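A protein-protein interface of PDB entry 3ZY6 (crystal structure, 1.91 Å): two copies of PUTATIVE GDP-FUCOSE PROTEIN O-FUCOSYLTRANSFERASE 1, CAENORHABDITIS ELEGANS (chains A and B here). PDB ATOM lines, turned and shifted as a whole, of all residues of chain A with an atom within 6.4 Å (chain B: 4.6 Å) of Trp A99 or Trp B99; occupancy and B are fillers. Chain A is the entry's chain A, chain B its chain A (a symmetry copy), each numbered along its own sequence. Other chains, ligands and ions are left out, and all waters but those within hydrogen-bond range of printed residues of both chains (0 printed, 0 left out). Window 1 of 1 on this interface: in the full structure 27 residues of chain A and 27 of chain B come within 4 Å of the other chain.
The side-chain sulfur (SG) of Cys A98 is disulfide-bonded to the side-chain sulfur (SG) of Cys A114 (2.0 Å). N of Gly A140 lies within hydrogen-bond range of O of Trp A99. O of Trp B99 lies within hydrogen-bond range of N of Gly B140.
Trp A99 touches Trp B99. Phe B146 touches Trp A99 (CZ to CZ3, 3.99 Å). Phe A146 touches Trp B99 (CZ to CZ3, 3.996 Å).
Printed residues of chain B within 4 Å of Trp A99: Trp B99 (3.7 Å) and Phe B146 (3.99 Å). Printed residues of chain B within 4 Å of Phe A146: Trp B99 (3.996 Å). Of the printed residues of chain A, Phe B146 touches Trp A99. The nearest printed residue of chain B that does not touch Phe A146 is Thr B100 (6.6 Å).
Printed residues of chain B that touch a printed residue of chain A: Trp B99 and Phe B146. Hydrophobic or aromatic side chains of chain A within 4 Å of the printed part of chain B: Trp A99 and Phe A146.
Trp A99 touches its own counterpart, Trp B99. Trp A99 touches Phe B146, and with the chains exchanged Phe A146 touches Trp B99. Of the 3 pairs that touch across the chains among the printed residues, 3 have their exchanged pair printed and touching as well.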
ATOM      1  N   PHE A  97     -15.417  -8.464   6.294  1.00  0.00           N
ATOM      2  CA  PHE A  97     -16.717  -8.622   5.670  1.00  0.00           C
ATOM      3  C   PHE A  97     -17.366  -9.875   6.198  1.00  0.00           C
ATOM      4  O   PHE A  97     -16.712 -10.913   6.315  1.00  0.00           O
ATOM      5  CB  PHE A  97     -16.612  -8.697   4.143  1.00  0.00           C
ATOM      6  CG  PHE A  97     -16.328  -7.379   3.493  1.00  0.00           C
ATOM      7  CD1 PHE A  97     -15.162  -6.681   3.793  1.00  0.00           C
ATOM      8  CD2 PHE A  97     -17.228  -6.832   2.583  1.00  0.00           C
ATOM      9  CE1 PHE A  97     -14.901  -5.455   3.202  1.00  0.00           C
ATOM     10  CE2 PHE A  97     -16.975  -5.606   1.979  1.00  0.00           C
ATOM     11  CZ  PHE A  97     -15.807  -4.920   2.291  1.00  0.00           C
ATOM     12  N   CYS A  98     -18.652  -9.764   6.529  1.00  0.00           N
ATOM     13  CA  CYS A  98     -19.437 -10.918   6.952  1.00  0.00           C
ATOM     14  C   CYS A  98     -20.924 -10.736   6.625  1.00  0.00           C
ATOM     15  O   CYS A  98     -21.348  -9.671   6.155  1.00  0.00           O
ATOM     16  CB  CYS A  98     -19.199 -11.245   8.431  1.00  0.00           C
ATOM     17  SG  CYS A  98     -19.695  -9.972   9.617  1.00  0.00           S
ATOM     18  N   TRP A  99     -21.699 -11.788   6.842  1.00  0.00           N
ATOM     19  CA  TRP A  99     -23.106 -11.802   6.475  1.00  0.00           C
ATOM     20  C   TRP A  99     -23.908 -10.780   7.282  1.00  0.00           C
ATOM     21  O   TRP A  99     -24.650  -9.972   6.716  1.00  0.00           O
ATOM     22  CB  TRP A  99     -23.673 -13.208   6.673  1.00  0.00           C
ATOM     23  CG  TRP A  99     -24.733 -13.562   5.678  1.00  0.00           C
ATOM     24  CD1 TRP A  99     -24.541 -14.114   4.440  1.00  0.00           C
ATOM     25  CD2 TRP A  99     -26.149 -13.382   5.825  1.00  0.00           C
ATOM     26  NE1 TRP A  99     -25.753 -14.291   3.807  1.00  0.00           N
ATOM     27  CE2 TRP A  99     -26.756 -13.854   4.634  1.00  0.00           C
ATOM     28  CE3 TRP A  99     -26.967 -12.870   6.848  1.00  0.00           C
ATOM     29  CZ2 TRP A  99     -28.146 -13.829   4.436  1.00  0.00           C
ATOM     30  CZ3 TRP A  99     -28.351 -12.847   6.652  1.00  0.00           C
ATOM     31  CH2 TRP A  99     -28.924 -13.326   5.453  1.00  0.00           C
ATOM     32  N   THR A 100     -23.728 -10.815   8.603  1.00  0.00           N
ATOM     33  CA  THR A 100     -24.506 -10.005   9.537  1.00  0.00           C
ATOM     34  C   THR A 100     -23.718  -9.800  10.833  1.00  0.00           C
ATOM     35  O   THR A 100     -22.851 -10.624  11.157  1.00  0.00           O
ATOM     36  CB  THR A 100     -25.916 -10.646   9.819  1.00  0.00           C
ATOM     37  OG1 THR A 100     -26.786  -9.679  10.412  1.00  0.00           O
ATOM     38  CG2 THR A 100     -25.834 -11.880  10.736  1.00  0.00           C
ATOM     39  N   PRO A 101     -24.001  -8.706  11.577  1.00  0.00           N
ATOM     40  CA  PRO A 101     -23.344  -8.577  12.874  1.00  0.00           C
ATOM     41  C   PRO A 101     -23.697  -9.786  13.735  1.00  0.00           C
ATOM     42  O   PRO A 101     -24.823 -10.294  13.654  1.00  0.00           O
ATOM     43  CB  PRO A 101     -23.960  -7.306  13.467  1.00  0.00           C
ATOM     44  CG  PRO A 101     -24.607  -6.597  12.349  1.00  0.00           C
ATOM     45  CD  PRO A 101     -24.972  -7.621  11.341  1.00  0.00           C
ATOM     46  N   ARG A 102     -22.741 -10.267  14.524  1.00  0.00           N
ATOM     47  CA  ARG A 102     -22.989 -11.451  15.354  1.00  0.00           C
ATOM     48  C   ARG A 102     -22.535 -11.273  16.794  1.00  0.00           C
ATOM     49  O   ARG A 102     -21.661 -10.455  17.092  1.00  0.00           O
ATOM     50  CB  ARG A 102     -22.344 -12.711  14.739  1.00  0.00           C
ATOM     51  CG  ARG A 102     -20.983 -13.091  15.342  1.00  0.00           C
ATOM     52  CD  ARG A 102     -20.304 -14.220  14.579  1.00  0.00           C
ATOM     53  NE  ARG A 102     -19.998 -13.811  13.210  1.00  0.00           N
ATOM     54  CZ  ARG A 102     -19.087 -14.387  12.427  1.00  0.00           C
ATOM     55  NH1 ARG A 102     -18.366 -15.408  12.881  1.00  0.00           N
ATOM     56  NH2 ARG A 102     -18.886 -13.928  11.188  1.00  0.00           N
ATOM     57  N   CYS A 114     -18.288  -8.844  13.059  1.00  0.00           N
ATOM     58  CA  CYS A 114     -17.839 -10.057  12.370  1.00  0.00           C
ATOM     59  C   CYS A 114     -16.979 -10.961  13.246  1.00  0.00           C
ATOM     60  O   CYS A 114     -16.976 -12.173  13.046  1.00  0.00           O
ATOM     61  CB  CYS A 114     -17.075  -9.706  11.095  1.00  0.00           C
ATOM     62  SG  CYS A 114     -18.057  -8.797   9.873  1.00  0.00           S
ATOM     63  N   GLU A 137     -18.008  -4.683   7.549  1.00  0.00           N
ATOM     64  CA  GLU A 137     -18.967  -4.474   6.478  1.00  0.00           C
ATOM     65  C   GLU A 137     -19.829  -5.720   6.371  1.00  0.00           C
ATOM     66  O   GLU A 137     -19.354  -6.834   6.617  1.00  0.00           O
ATOM     67  CB  GLU A 137     -18.254  -4.192   5.154  1.00  0.00           C
ATOM     68  CG  GLU A 137     -17.469  -2.865   5.105  1.00  0.00           C
ATOM     69  CD  GLU A 137     -18.347  -1.626   4.825  1.00  0.00           C
ATOM     70  OE1 GLU A 137     -19.519  -1.775   4.384  1.00  0.00           O
ATOM     71  OE2 GLU A 137     -17.841  -0.497   5.029  1.00  0.00           O
ATOM     72  N   TYR A 138     -21.096  -5.539   6.015  1.00  0.00           N
ATOM     73  CA  TYR A 138     -22.020  -6.667   5.944  1.00  0.00           C
ATOM     74  C   TYR A 138     -22.641  -6.802   4.561  1.00  0.00           C
ATOM     75  O   TYR A 138     -22.853  -5.803   3.870  1.00  0.00           O
ATOM     76  CB  TYR A 138     -23.097  -6.547   7.029  1.00  0.00           C
ATOM     77  CG  TYR A 138     -22.539  -6.198   8.393  1.00  0.00           C
ATOM     78  CD1 TYR A 138     -21.942  -7.175   9.200  1.00  0.00           C
ATOM     79  CD2 TYR A 138     -22.612  -4.893   8.884  1.00  0.00           C
ATOM     80  CE1 TYR A 138     -21.420  -6.853  10.456  1.00  0.00           C
ATOM     81  CE2 TYR A 138     -22.102  -4.564  10.148  1.00  0.00           C
ATOM     82  CZ  TYR A 138     -21.508  -5.547  10.925  1.00  0.00           C
ATOM     83  OH  TYR A 138     -21.006  -5.227  12.166  1.00  0.00           O
ATOM     84  N   PHE A 139     -22.913  -8.038   4.148  1.00  0.00           N
ATOM     85  CA  PHE A 139     -23.455  -8.283   2.808  1.00  0.00           C
ATOM     86  C   PHE A 139     -24.736  -9.124   2.804  1.00  0.00           C
ATOM     87  O   PHE A 139     -25.276  -9.450   1.733  1.00  0.00           O
ATOM     88  CB  PHE A 139     -22.389  -8.909   1.893  1.00  0.00           C
ATOM     89  CG  PHE A 139     -21.788 -10.182   2.432  1.00  0.00           C
ATOM     90  CD1 PHE A 139     -22.471 -11.394   2.324  1.00  0.00           C
ATOM     91  CD2 PHE A 139     -20.530 -10.170   3.035  1.00  0.00           C
ATOM     92  CE1 PHE A 139     -21.928 -12.560   2.821  1.00  0.00           C
ATOM     93  CE2 PHE A 139     -19.970 -11.345   3.531  1.00  0.00           C
ATOM     94  CZ  PHE A 139     -20.664 -12.537   3.430  1.00  0.00           C
ATOM     95  N   GLY A 140     -25.221  -9.455   3.999  1.00  0.00           N
ATOM     96  CA  GLY A 140     -26.445 -10.239   4.169  1.00  0.00           C
ATOM     97  C   GLY A 140     -27.680  -9.571   3.598  1.00  0.00           C
ATOM     98  O   GLY A 140     -28.634 -10.246   3.226  1.00  0.00           O
ATOM     99  N   ASP A 141     -27.644  -8.242   3.526  1.00  0.00           N
ATOM    100  CA  ASP A 141     -28.715  -7.428   2.950  1.00  0.00           C
ATOM    101  C   ASP A 141     -28.707  -7.359   1.405  1.00  0.00           C
ATOM    102  O   ASP A 141     -29.606  -6.767   0.801  1.00  0.00           O
ATOM    103  CB  ASP A 141     -28.708  -6.015   3.573  1.00  0.00           C
ATOM    104  CG  ASP A 141     -27.326  -5.346   3.548  1.00  0.00           C
ATOM    105  OD1 ASP A 141     -26.290  -6.024   3.772  1.00  0.00           O
ATOM    106  OD2 ASP A 141     -27.275  -4.123   3.312  1.00  0.00           O
ATOM    107  N   ILE A 142     -27.702  -7.960   0.770  1.00  0.00           N
ATOM    108  CA  ILE A 142     -27.646  -8.019  -0.698  1.00  0.00           C
ATOM    109  C   ILE A 142     -28.506  -9.191  -1.205  1.00  0.00           C
ATOM    110  O   ILE A 142     -28.308 -10.333  -0.773  1.00  0.00           O
ATOM    111  CB  ILE A 142     -26.174  -8.105  -1.241  1.00  0.00           C
ATOM    112  CG1 ILE A 142     -25.359  -6.881  -0.801  1.00  0.00           C
ATOM    113  CG2 ILE A 142     -26.155  -8.243  -2.769  1.00  0.00           C
ATOM    114  CD1 ILE A 142     -23.909  -6.869  -1.293  1.00  0.00           C
ATOM    115  N   GLY A 145     -27.198 -13.123  -1.714  1.00  0.00           N
ATOM    116  CA  GLY A 145     -25.983 -13.464  -0.976  1.00  0.00           C
ATOM    117  C   GLY A 145     -24.761 -13.444  -1.876  1.00  0.00           C
ATOM    118  O   GLY A 145     -24.622 -12.560  -2.735  1.00  0.00           O
ATOM    119  N   PHE A 146     -23.884 -14.430  -1.687  1.00  0.00           N
ATOM    120  CA  PHE A 146     -22.699 -14.589  -2.540  1.00  0.00           C
ATOM    121  C   PHE A 146     -22.890 -15.588  -3.698  1.00  0.00           C
ATOM    122  O   PHE A 146     -21.913 -16.077  -4.268  1.00  0.00           O
ATOM    123  CB  PHE A 146     -21.436 -14.907  -1.712  1.00  0.00           C
ATOM    124  CG  PHE A 146     -21.615 -15.980  -0.661  1.00  0.00           C
ATOM    125  CD1 PHE A 146     -22.149 -17.227  -0.982  1.00  0.00           C
ATOM    126  CD2 PHE A 146     -21.194 -15.754   0.645  1.00  0.00           C
ATOM    127  CE1 PHE A 146     -22.290 -18.215  -0.015  1.00  0.00           C
ATOM    128  CE2 PHE A 146     -21.329 -16.735   1.621  1.00  0.00           C
ATOM    129  CZ  PHE A 146     -21.875 -17.969   1.290  1.00  0.00           C
ATOM    130  N   PRO A 177     -20.558 -21.613  -0.721  1.00  0.00           N
ATOM    131  CA  PRO A 177     -21.277 -22.663   0.004  1.00  0.00           C
ATOM    132  C   PRO A 177     -20.378 -23.800   0.479  1.00  0.00           C
ATOM    133  O   PRO A 177     -19.308 -24.063  -0.093  1.00  0.00           O
ATOM    134  CB  PRO A 177     -22.275 -23.188  -1.027  1.00  0.00           C
ATOM    135  CG  PRO A 177     -22.463 -22.057  -1.998  1.00  0.00           C
ATOM    136  CD  PRO A 177     -21.125 -21.374  -2.061  1.00  0.00           C
ATOM    137  N   CYS B  98     -29.705 -23.711  11.135  1.00  0.00           N
ATOM    138  CA  CYS B  98     -28.804 -22.591  10.885  1.00  0.00           C
ATOM    139  C   CYS B  98     -28.532 -22.415   9.386  1.00  0.00           C
ATOM    140  O   CYS B  98     -28.971 -23.224   8.558  1.00  0.00           O
ATOM    141  CB  CYS B  98     -27.514 -22.717  11.704  1.00  0.00           C
ATOM    142  SG  CYS B  98     -26.474 -24.151  11.336  1.00  0.00           S
ATOM    143  N   TRP B  99     -27.838 -21.338   9.046  1.00  0.00           N
ATOM    144  CA  TRP B  99     -27.599 -20.979   7.657  1.00  0.00           C
ATOM    145  C   TRP B  99     -26.732 -22.019   6.948  1.00  0.00           C
ATOM    146  O   TRP B  99     -27.084 -22.504   5.869  1.00  0.00           O
ATOM    147  CB  TRP B  99     -26.944 -19.598   7.591  1.00  0.00           C
ATOM    148  CG  TRP B  99     -27.349 -18.811   6.385  1.00  0.00           C
ATOM    149  CD1 TRP B  99     -28.440 -17.993   6.270  1.00  0.00           C
ATOM    150  CD2 TRP B  99     -26.678 -18.770   5.116  1.00  0.00           C
ATOM    151  NE1 TRP B  99     -28.490 -17.443   5.006  1.00  0.00           N
ATOM    152  CE2 TRP B  99     -27.420 -17.900   4.279  1.00  0.00           C
ATOM    153  CE3 TRP B  99     -25.520 -19.383   4.604  1.00  0.00           C
ATOM    154  CZ2 TRP B  99     -27.042 -17.625   2.955  1.00  0.00           C
ATOM    155  CZ3 TRP B  99     -25.143 -19.108   3.287  1.00  0.00           C
ATOM    156  CH2 TRP B  99     -25.904 -18.234   2.479  1.00  0.00           C
ATOM    157  N   THR B 100     -25.612 -22.369   7.582  1.00  0.00           N
ATOM    158  CA  THR B 100     -24.603 -23.248   6.996  1.00  0.00           C
ATOM    159  C   THR B 100     -23.792 -23.926   8.103  1.00  0.00           C
ATOM    160  O   THR B 100     -23.705 -23.384   9.214  1.00  0.00           O
ATOM    161  CB  THR B 100     -23.669 -22.466   5.999  1.00  0.00           C
ATOM    162  OG1 THR B 100     -22.956 -23.387   5.168  1.00  0.00           O
ATOM    163  CG2 THR B 100     -22.660 -21.554   6.722  1.00  0.00           C
ATOM    164  N   TYR B 138     -29.929 -27.147   7.637  1.00  0.00           N
ATOM    165  CA  TYR B 138     -29.421 -25.896   7.082  1.00  0.00           C
ATOM    166  C   TYR B 138     -30.389 -25.291   6.076  1.00  0.00           C
ATOM    167  O   TYR B 138     -31.101 -26.016   5.377  1.00  0.00           O
ATOM    168  CB  TYR B 138     -28.034 -26.107   6.463  1.00  0.00           C
ATOM    169  CG  TYR B 138     -27.095 -26.899   7.350  1.00  0.00           C
ATOM    170  CD1 TYR B 138     -26.439 -26.294   8.428  1.00  0.00           C
ATOM    171  CD2 TYR B 138     -26.855 -28.254   7.109  1.00  0.00           C
ATOM    172  CE1 TYR B 138     -25.578 -27.024   9.252  1.00  0.00           C
ATOM    173  CE2 TYR B 138     -25.984 -28.992   7.922  1.00  0.00           C
ATOM    174  CZ  TYR B 138     -25.352 -28.371   8.990  1.00  0.00           C
ATOM    175  OH  TYR B 138     -24.495 -29.093   9.791  1.00  0.00           O
ATOM    176  N   PHE B 139     -30.432 -23.962   6.015  1.00  0.00           N
ATOM    177  CA  PHE B 139     -31.374 -23.277   5.124  1.00  0.00           C
ATOM    178  C   PHE B 139     -30.713 -22.253   4.195  1.00  0.00           C
ATOM    179  O   PHE B 139     -31.400 -21.564   3.422  1.00  0.00           O
ATOM    180  CB  PHE B 139     -32.514 -22.630   5.927  1.00  0.00           C
ATOM    181  CG  PHE B 139     -32.047 -21.672   6.994  1.00  0.00           C
ATOM    182  CD1 PHE B 139     -31.655 -20.374   6.665  1.00  0.00           C
ATOM    183  CD2 PHE B 139     -32.014 -22.066   8.331  1.00  0.00           C
ATOM    184  CE1 PHE B 139     -31.222 -19.497   7.636  1.00  0.00           C
ATOM    185  CE2 PHE B 139     -31.587 -21.184   9.320  1.00  0.00           C
ATOM    186  CZ  PHE B 139     -31.187 -19.905   8.978  1.00  0.00           C
ATOM    187  N   GLY B 140     -29.386 -22.171   4.267  1.00  0.00           N
ATOM    188  CA  GLY B 140     -28.602 -21.257   3.435  1.00  0.00           C
ATOM    189  C   GLY B 140     -28.735 -21.520   1.948  1.00  0.00           C
ATOM    190  O   GLY B 140     -28.566 -20.612   1.140  1.00  0.00           O
ATOM    191  N   PHE B 146     -34.151 -16.181   4.797  1.00  0.00           N
ATOM    192  CA  PHE B 146     -35.366 -16.013   5.604  1.00  0.00           C
ATOM    193  C   PHE B 146     -36.153 -14.725   5.293  1.00  0.00           C
ATOM    194  O   PHE B 146     -36.973 -14.283   6.100  1.00  0.00           O
ATOM    195  CB  PHE B 146     -35.076 -16.156   7.113  1.00  0.00           C
ATOM    196  CG  PHE B 146     -33.870 -15.386   7.606  1.00  0.00           C
ATOM    197  CD1 PHE B 146     -33.723 -14.024   7.345  1.00  0.00           C
ATOM    198  CD2 PHE B 146     -32.907 -16.022   8.382  1.00  0.00           C
ATOM    199  CE1 PHE B 146     -32.623 -13.320   7.819  1.00  0.00           C
ATOM    200  CE2 PHE B 146     -31.802 -15.328   8.863  1.00  0.00           C
ATOM    201  CZ  PHE B 146     -31.661 -13.974   8.584  1.00  0.00           C
